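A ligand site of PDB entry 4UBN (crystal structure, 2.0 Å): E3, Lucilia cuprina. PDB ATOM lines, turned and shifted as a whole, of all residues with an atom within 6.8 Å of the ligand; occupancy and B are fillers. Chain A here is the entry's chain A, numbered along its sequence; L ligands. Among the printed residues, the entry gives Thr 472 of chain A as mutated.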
ATOM      1  N   HIS A 134      26.577  24.844  14.952  1.00  0.00           N
ATOM      2  CA  HIS A 134      25.174  24.519  14.717  1.00  0.00           C
ATOM      3  C   HIS A 134      24.706  24.985  13.330  1.00  0.00           C
ATOM      4  O   HIS A 134      25.258  25.925  12.777  1.00  0.00           O
ATOM      5  CB  HIS A 134      24.290  25.136  15.797  1.00  0.00           C
ATOM      6  CG  HIS A 134      24.139  26.627  15.666  1.00  0.00           C
ATOM      7  ND1 HIS A 134      23.343  27.217  14.703  1.00  0.00           N
ATOM      8  CD2 HIS A 134      24.666  27.635  16.392  1.00  0.00           C
ATOM      9  CE1 HIS A 134      23.387  28.529  14.842  1.00  0.00           C
ATOM     10  NE2 HIS A 134      24.179  28.815  15.858  1.00  0.00           N
ATOM     11  N   GLY A 135      23.693  24.315  12.787  1.00  0.00           N
ATOM     12  CA  GLY A 135      23.079  24.718  11.531  1.00  0.00           C
ATOM     13  C   GLY A 135      21.905  25.626  11.827  1.00  0.00           C
ATOM     14  O   GLY A 135      21.767  26.117  12.942  1.00  0.00           O
ATOM     15  N   GLY A 136      21.052  25.841  10.834  1.00  0.00           N
ATOM     16  CA  GLY A 136      19.969  26.798  10.982  1.00  0.00           C
ATOM     17  C   GLY A 136      19.998  27.838   9.870  1.00  0.00           C
ATOM     18  O   GLY A 136      19.608  28.992  10.069  1.00  0.00           O
ATOM     19  N   GLY A 137      20.497  27.404   8.713  1.00  0.00           N
ATOM     20  CA  GLY A 137      20.487  28.205   7.497  1.00  0.00           C
ATOM     21  C   GLY A 137      21.247  29.501   7.605  1.00  0.00           C
ATOM     22  O   GLY A 137      21.067  30.387   6.761  1.00  0.00           O
ATOM     23  N   PHE A 138      22.077  29.609   8.637  1.00  0.00           N
ATOM     24  CA  PHE A 138      22.833  30.824   8.974  1.00  0.00           C
ATOM     25  C   PHE A 138      21.940  31.946   9.476  1.00  0.00           C
ATOM     26  O   PHE A 138      22.370  33.103   9.535  1.00  0.00           O
ATOM     27  CB  PHE A 138      23.641  31.349   7.787  1.00  0.00           C
ATOM     28  CG  PHE A 138      24.715  30.408   7.296  1.00  0.00           C
ATOM     29  CD1 PHE A 138      25.899  30.288   7.983  1.00  0.00           C
ATOM     30  CD2 PHE A 138      24.536  29.682   6.138  1.00  0.00           C
ATOM     31  CE1 PHE A 138      26.905  29.441   7.513  1.00  0.00           C
ATOM     32  CE2 PHE A 138      25.535  28.825   5.661  1.00  0.00           C
ATOM     33  CZ  PHE A 138      26.720  28.700   6.357  1.00  0.00           C
ATOM     34  N   ILE A 140      19.163  31.086  12.087  1.00  0.00           N
ATOM     35  CA  ILE A 140      18.684  30.722  13.415  1.00  0.00           C
ATOM     36  C   ILE A 140      19.696  29.791  14.082  1.00  0.00           C
ATOM     37  O   ILE A 140      20.580  29.247  13.416  1.00  0.00           O
ATOM     38  CB  ILE A 140      17.303  29.997  13.406  1.00  0.00           C
ATOM     39  CG1 ILE A 140      17.404  28.680  12.643  1.00  0.00           C
ATOM     40  CG2 ILE A 140      16.178  30.900  12.855  1.00  0.00           C
ATOM     41  CD1 ILE A 140      16.332  27.727  12.974  1.00  0.00           C
ATOM     42  N   GLU A 217      26.132  20.402  11.306  1.00  0.00           N
ATOM     43  CA  GLU A 217      25.043  19.870  10.501  1.00  0.00           C
ATOM     44  C   GLU A 217      24.366  21.016   9.730  1.00  0.00           C
ATOM     45  O   GLU A 217      24.229  22.111  10.249  1.00  0.00           O
ATOM     46  CB  GLU A 217      24.071  19.103  11.406  1.00  0.00           C
ATOM     47  CG  GLU A 217      23.047  18.266  10.671  1.00  0.00           C
ATOM     48  CD  GLU A 217      21.743  19.014  10.477  1.00  0.00           C
ATOM     49  OE1 GLU A 217      21.569  20.075  11.116  1.00  0.00           O
ATOM     50  OE2 GLU A 217      20.894  18.558   9.678  1.00  0.00           O
ATOM     51  N   SER A 218      23.965  20.745   8.487  1.00  0.00           N
ATOM     52  CA  SER A 218      23.327  21.735   7.607  1.00  0.00           C
ATOM     53  C   SER A 218      24.221  22.965   7.389  1.00  0.00           C
ATOM     54  O   SER A 218      25.349  22.841   6.905  1.00  0.00           O
ATOM     55  CB  SER A 218      21.961  22.134   8.183  1.00  0.00           C
ATOM     56  OG  SER A 218      21.217  22.870   7.239  1.00  0.00           O
ATOM     57  N   ALA A 219      23.740  24.150   7.768  1.00  0.00           N
ATOM     58  CA  ALA A 219      24.565  25.358   7.712  1.00  0.00           C
ATOM     59  C   ALA A 219      25.815  25.196   8.567  1.00  0.00           C
ATOM     60  O   ALA A 219      26.809  25.845   8.325  1.00  0.00           O
ATOM     61  CB  ALA A 219      23.764  26.599   8.181  1.00  0.00           C
ATOM     62  N   GLY A 220      25.750  24.329   9.580  1.00  0.00           N
ATOM     63  CA  GLY A 220      26.914  24.029  10.399  1.00  0.00           C
ATOM     64  C   GLY A 220      27.899  23.132   9.674  1.00  0.00           C
ATOM     65  O   GLY A 220      29.104  23.183   9.941  1.00  0.00           O
ATOM     66  N   ALA A 221      27.387  22.313   8.754  1.00  0.00           N
ATOM     67  CA  ALA A 221      28.240  21.515   7.884  1.00  0.00           C
ATOM     68  C   ALA A 221      28.925  22.392   6.848  1.00  0.00           C
ATOM     69  O   ALA A 221      30.119  22.258   6.605  1.00  0.00           O
ATOM     70  CB  ALA A 221      27.445  20.397   7.214  1.00  0.00           C
ATOM     71  N   SER A 244      25.239  16.409   6.321  1.00  0.00           N
ATOM     72  CA  SER A 244      24.176  16.997   5.505  1.00  0.00           C
ATOM     73  C   SER A 244      24.527  18.391   5.014  1.00  0.00           C
ATOM     74  O   SER A 244      23.730  19.321   5.168  1.00  0.00           O
ATOM     75  CB  SER A 244      22.853  17.071   6.278  1.00  0.00           C
ATOM     76  OG  SER A 244      22.258  15.800   6.449  1.00  0.00           O
ATOM     77  N   TRP A 251      22.521  26.510  -1.390  1.00  0.00           N
ATOM     78  CA  TRP A 251      22.055  27.370  -0.311  1.00  0.00           C
ATOM     79  C   TRP A 251      23.185  27.933   0.578  1.00  0.00           C
ATOM     80  O   TRP A 251      22.941  28.805   1.414  1.00  0.00           O
ATOM     81  CB  TRP A 251      21.067  26.597   0.569  1.00  0.00           C
ATOM     82  CG  TRP A 251      21.582  25.245   0.951  1.00  0.00           C
ATOM     83  CD1 TRP A 251      21.329  24.062   0.312  1.00  0.00           C
ATOM     84  CD2 TRP A 251      22.442  24.936   2.053  1.00  0.00           C
ATOM     85  NE1 TRP A 251      21.975  23.027   0.950  1.00  0.00           N
ATOM     86  CE2 TRP A 251      22.667  23.541   2.027  1.00  0.00           C
ATOM     87  CE3 TRP A 251      23.047  25.701   3.053  1.00  0.00           C
ATOM     88  CZ2 TRP A 251      23.488  22.894   2.958  1.00  0.00           C
ATOM     89  CZ3 TRP A 251      23.846  25.047   4.004  1.00  0.00           C
ATOM     90  CH2 TRP A 251      24.064  23.659   3.937  1.00  0.00           C
ATOM     91  N   MET A 308      17.712  30.622  -1.319  1.00  0.00           N
ATOM     92  CA  MET A 308      16.994  30.251  -0.097  1.00  0.00           C
ATOM     93  C   MET A 308      17.003  31.341   0.981  1.00  0.00           C
ATOM     94  O   MET A 308      16.006  31.522   1.683  1.00  0.00           O
ATOM     95  CB  MET A 308      17.558  28.932   0.460  1.00  0.00           C
ATOM     96  CG  MET A 308      16.632  28.288   1.487  1.00  0.00           C
ATOM     97  SD  MET A 308      17.327  26.812   2.271  1.00  0.00           S
ATOM     98  CE  MET A 308      17.048  25.598   0.990  1.00  0.00           C
ATOM     99  N   PHE A 309      18.124  32.057   1.111  1.00  0.00           N
ATOM    100  CA  PHE A 309      18.255  33.100   2.125  1.00  0.00           C
ATOM    101  C   PHE A 309      18.831  34.386   1.519  1.00  0.00           C
ATOM    102  O   PHE A 309      19.741  34.324   0.692  1.00  0.00           O
ATOM    103  CB  PHE A 309      19.177  32.633   3.251  1.00  0.00           C
ATOM    104  CG  PHE A 309      18.867  31.261   3.775  1.00  0.00           C
ATOM    105  CD1 PHE A 309      17.801  31.050   4.644  1.00  0.00           C
ATOM    106  CD2 PHE A 309      19.659  30.181   3.427  1.00  0.00           C
ATOM    107  CE1 PHE A 309      17.510  29.785   5.146  1.00  0.00           C
ATOM    108  CE2 PHE A 309      19.381  28.907   3.934  1.00  0.00           C
ATOM    109  CZ  PHE A 309      18.308  28.717   4.803  1.00  0.00           C
ATOM    110  N   PHE A 354      12.147  16.583   4.649  1.00  0.00           N
ATOM    111  CA  PHE A 354      12.053  17.832   5.386  1.00  0.00           C
ATOM    112  C   PHE A 354      11.049  18.835   4.792  1.00  0.00           C
ATOM    113  O   PHE A 354      10.278  19.461   5.508  1.00  0.00           O
ATOM    114  CB  PHE A 354      13.460  18.455   5.464  1.00  0.00           C
ATOM    115  CG  PHE A 354      13.553  19.668   6.321  1.00  0.00           C
ATOM    116  CD1 PHE A 354      13.502  20.931   5.755  1.00  0.00           C
ATOM    117  CD2 PHE A 354      13.727  19.558   7.698  1.00  0.00           C
ATOM    118  CE1 PHE A 354      13.601  22.067   6.536  1.00  0.00           C
ATOM    119  CE2 PHE A 354      13.836  20.692   8.489  1.00  0.00           C
ATOM    120  CZ  PHE A 354      13.759  21.942   7.906  1.00  0.00           C
ATOM    121  N   PHE A 355      11.034  18.957   3.471  1.00  0.00           N
ATOM    122  CA  PHE A 355      10.260  20.000   2.809  1.00  0.00           C
ATOM    123  C   PHE A 355       8.760  19.789   2.753  1.00  0.00           C
ATOM    124  O   PHE A 355       8.078  20.510   2.015  1.00  0.00           O
ATOM    125  CB  PHE A 355      10.778  20.204   1.381  1.00  0.00           C
ATOM    126  CG  PHE A 355      12.139  20.794   1.330  1.00  0.00           C
ATOM    127  CD1 PHE A 355      12.318  22.158   1.524  1.00  0.00           C
ATOM    128  CD2 PHE A 355      13.248  19.999   1.132  1.00  0.00           C
ATOM    129  CE1 PHE A 355      13.584  22.705   1.499  1.00  0.00           C
ATOM    130  CE2 PHE A 355      14.514  20.551   1.098  1.00  0.00           C
ATOM    131  CZ  PHE A 355      14.673  21.913   1.281  1.00  0.00           C
ATOM    132  N   TYR A 420      19.776  19.743  -2.919  1.00  0.00           N
ATOM    133  CA  TYR A 420      20.317  20.455  -1.786  1.00  0.00           C
ATOM    134  C   TYR A 420      21.499  19.769  -1.120  1.00  0.00           C
ATOM    135  O   TYR A 420      22.307  20.447  -0.506  1.00  0.00           O
ATOM    136  CB  TYR A 420      19.214  20.701  -0.736  1.00  0.00           C
ATOM    137  CG  TYR A 420      18.163  21.672  -1.220  1.00  0.00           C
ATOM    138  CD1 TYR A 420      18.483  23.013  -1.443  1.00  0.00           C
ATOM    139  CD2 TYR A 420      16.866  21.261  -1.462  1.00  0.00           C
ATOM    140  CE1 TYR A 420      17.528  23.917  -1.910  1.00  0.00           C
ATOM    141  CE2 TYR A 420      15.895  22.145  -1.928  1.00  0.00           C
ATOM    142  CZ  TYR A 420      16.229  23.481  -2.153  1.00  0.00           C
ATOM    143  OH  TYR A 420      15.268  24.360  -2.601  1.00  0.00           O
ATOM    144  N   PHE A 421      21.620  18.444  -1.262  1.00  0.00           N
ATOM    145  CA  PHE A 421      22.624  17.703  -0.481  1.00  0.00           C
ATOM    146  C   PHE A 421      23.502  16.708  -1.265  1.00  0.00           C
ATOM    147  O   PHE A 421      24.735  16.859  -1.287  1.00  0.00           O
ATOM    148  CB  PHE A 421      21.916  16.996   0.672  1.00  0.00           C
ATOM    149  CG  PHE A 421      21.147  17.937   1.570  1.00  0.00           C
ATOM    150  CD1 PHE A 421      21.815  18.788   2.443  1.00  0.00           C
ATOM    151  CD2 PHE A 421      19.757  17.988   1.526  1.00  0.00           C
ATOM    152  CE1 PHE A 421      21.111  19.673   3.250  1.00  0.00           C
ATOM    153  CE2 PHE A 421      19.053  18.873   2.333  1.00  0.00           C
ATOM    154  CZ  PHE A 421      19.736  19.720   3.181  1.00  0.00           C
ATOM    155  N   TYR A 457      13.304  20.219  15.472  1.00  0.00           N
ATOM    156  CA  TYR A 457      13.159  20.431  14.023  1.00  0.00           C
ATOM    157  C   TYR A 457      11.970  19.665  13.449  1.00  0.00           C
ATOM    158  O   TYR A 457      11.441  20.014  12.399  1.00  0.00           O
ATOM    159  CB  TYR A 457      14.434  20.026  13.278  1.00  0.00           C
ATOM    160  CG  TYR A 457      15.505  21.092  13.270  1.00  0.00           C
ATOM    161  CD1 TYR A 457      15.396  22.202  12.430  1.00  0.00           C
ATOM    162  CD2 TYR A 457      16.624  20.985  14.081  1.00  0.00           C
ATOM    163  CE1 TYR A 457      16.373  23.174  12.410  1.00  0.00           C
ATOM    164  CE2 TYR A 457      17.611  21.960  14.062  1.00  0.00           C
ATOM    165  CZ  TYR A 457      17.478  23.047  13.222  1.00  0.00           C
ATOM    166  OH  TYR A 457      18.445  24.025  13.183  1.00  0.00           O
ATOM    167  N   MET A 460       9.182  22.036  13.371  1.00  0.00           N
ATOM    168  CA  MET A 460       9.305  22.986  12.275  1.00  0.00           C
ATOM    169  C   MET A 460       8.858  22.363  10.946  1.00  0.00           C
ATOM    170  O   MET A 460       8.003  22.913  10.270  1.00  0.00           O
ATOM    171  CB  MET A 460      10.754  23.466  12.182  1.00  0.00           C
ATOM    172  CG  MET A 460      11.010  24.473  11.065  1.00  0.00           C
ATOM    173  SD  MET A 460      12.772  24.866  10.865  1.00  0.00           S
ATOM    174  CE  MET A 460      13.136  25.588  12.456  1.00  0.00           C
ATOM    175  N   HIS A 471      16.332  15.184   6.928  1.00  0.00           N
ATOM    176  CA  HIS A 471      17.316  16.183   7.321  1.00  0.00           C
ATOM    177  C   HIS A 471      17.056  16.568   8.793  1.00  0.00           C
ATOM    178  O   HIS A 471      15.910  16.860   9.140  1.00  0.00           O
ATOM    179  CB  HIS A 471      17.206  17.399   6.379  1.00  0.00           C
ATOM    180  CG  HIS A 471      18.254  18.444   6.588  1.00  0.00           C
ATOM    181  ND1 HIS A 471      19.578  18.249   6.250  1.00  0.00           N
ATOM    182  CD2 HIS A 471      18.171  19.696   7.087  1.00  0.00           C
ATOM    183  CE1 HIS A 471      20.268  19.331   6.553  1.00  0.00           C
ATOM    184  NE2 HIS A 471      19.444  20.227   7.053  1.00  0.00           N
ATOM    185  N   THR A 472      18.106  16.526   9.631  1.00  0.00           N
ATOM    186  CA  THR A 472      18.100  16.901  11.075  1.00  0.00           C
ATOM    187  C   THR A 472      17.647  15.813  12.055  1.00  0.00           C
ATOM    188  O   THR A 472      17.725  16.009  13.272  1.00  0.00           O
ATOM    189  CB  THR A 472      17.206  18.116  11.432  1.00  0.00           C
ATOM    190  OG1 THR A 472      15.831  17.736  11.359  1.00  0.00           O
ATOM    191  CG2 THR A 472      17.481  19.315  10.532  1.00  0.00           C
HETATM  192  O1  LIG L   1      21.105  24.659   8.201  1.00  0.00           O
HETATM  193  P1  LIG L   1      20.123  23.847   7.409  1.00  0.00           P
HETATM  194  O2  LIG L   1      19.844  24.694   6.014  1.00  0.00           O
HETATM  195  C1  LIG L   1      20.256  24.120   4.842  1.00  0.00           C
HETATM  196  C2  LIG L   1      19.180  24.341   3.818  1.00  0.00           C
HETATM  197  O3  LIG L   1      18.703  24.029   8.223  1.00  0.00           O
HETATM  198  C3  LIG L   1      18.487  23.226   9.312  1.00  0.00           C
HETATM  199  C4  LIG L   1      17.225  22.448   9.053  1.00  0.00           C
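The backbone NH of Gly 137 sits at hydrogen-bond distance from an oxygen (O1) of the ligand. O1 of the ligand sits at hydrogen-bond distance from N of Ala 219 (2.7 Å). An oxygen (O1) of the ligand lies within hydrogen-bond range of the backbone NH (N) of Gly 136. OG of Ser 218 is bonded to P1 of the ligand (1.5 Å).
The backbone NH of Gly 135 lies close to the backbone carbonyl oxygen of Glu 217, 3.4 Å away. A ring nitrogen (NE2) of His 471 lies close to the side-chain carboxylate (OE2) of Glu 217, at 3.4 Å. NE2 of His 471 lies within hydrogen-bond range of OG of Ser 218. N of Thr 472 lies within hydrogen-bond range of OE2 of Glu 217, 3.5 Å away. O of Tyr 420 sits at hydrogen-bond distance from NE1 of Trp 251.
C of Gly 135 touches O1 of the ligand (3.8 Å). Trp 251 touches the ligand (CD2 to C1, 3.6 Å). SD of Met 308 touches C2 of the ligand (3.5 Å). CZ of Phe 354 touches C4 of the ligand, 3.7 Å away. Tyr 457 touches the ligand. CD2 of His 471 touches C4 of the ligand (3.5 Å). CG2 of Thr 472 touches C4 of the ligand (3.5 Å). The nearest printed residue that does not touch the ligand is Phe 309 (4.5 Å).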
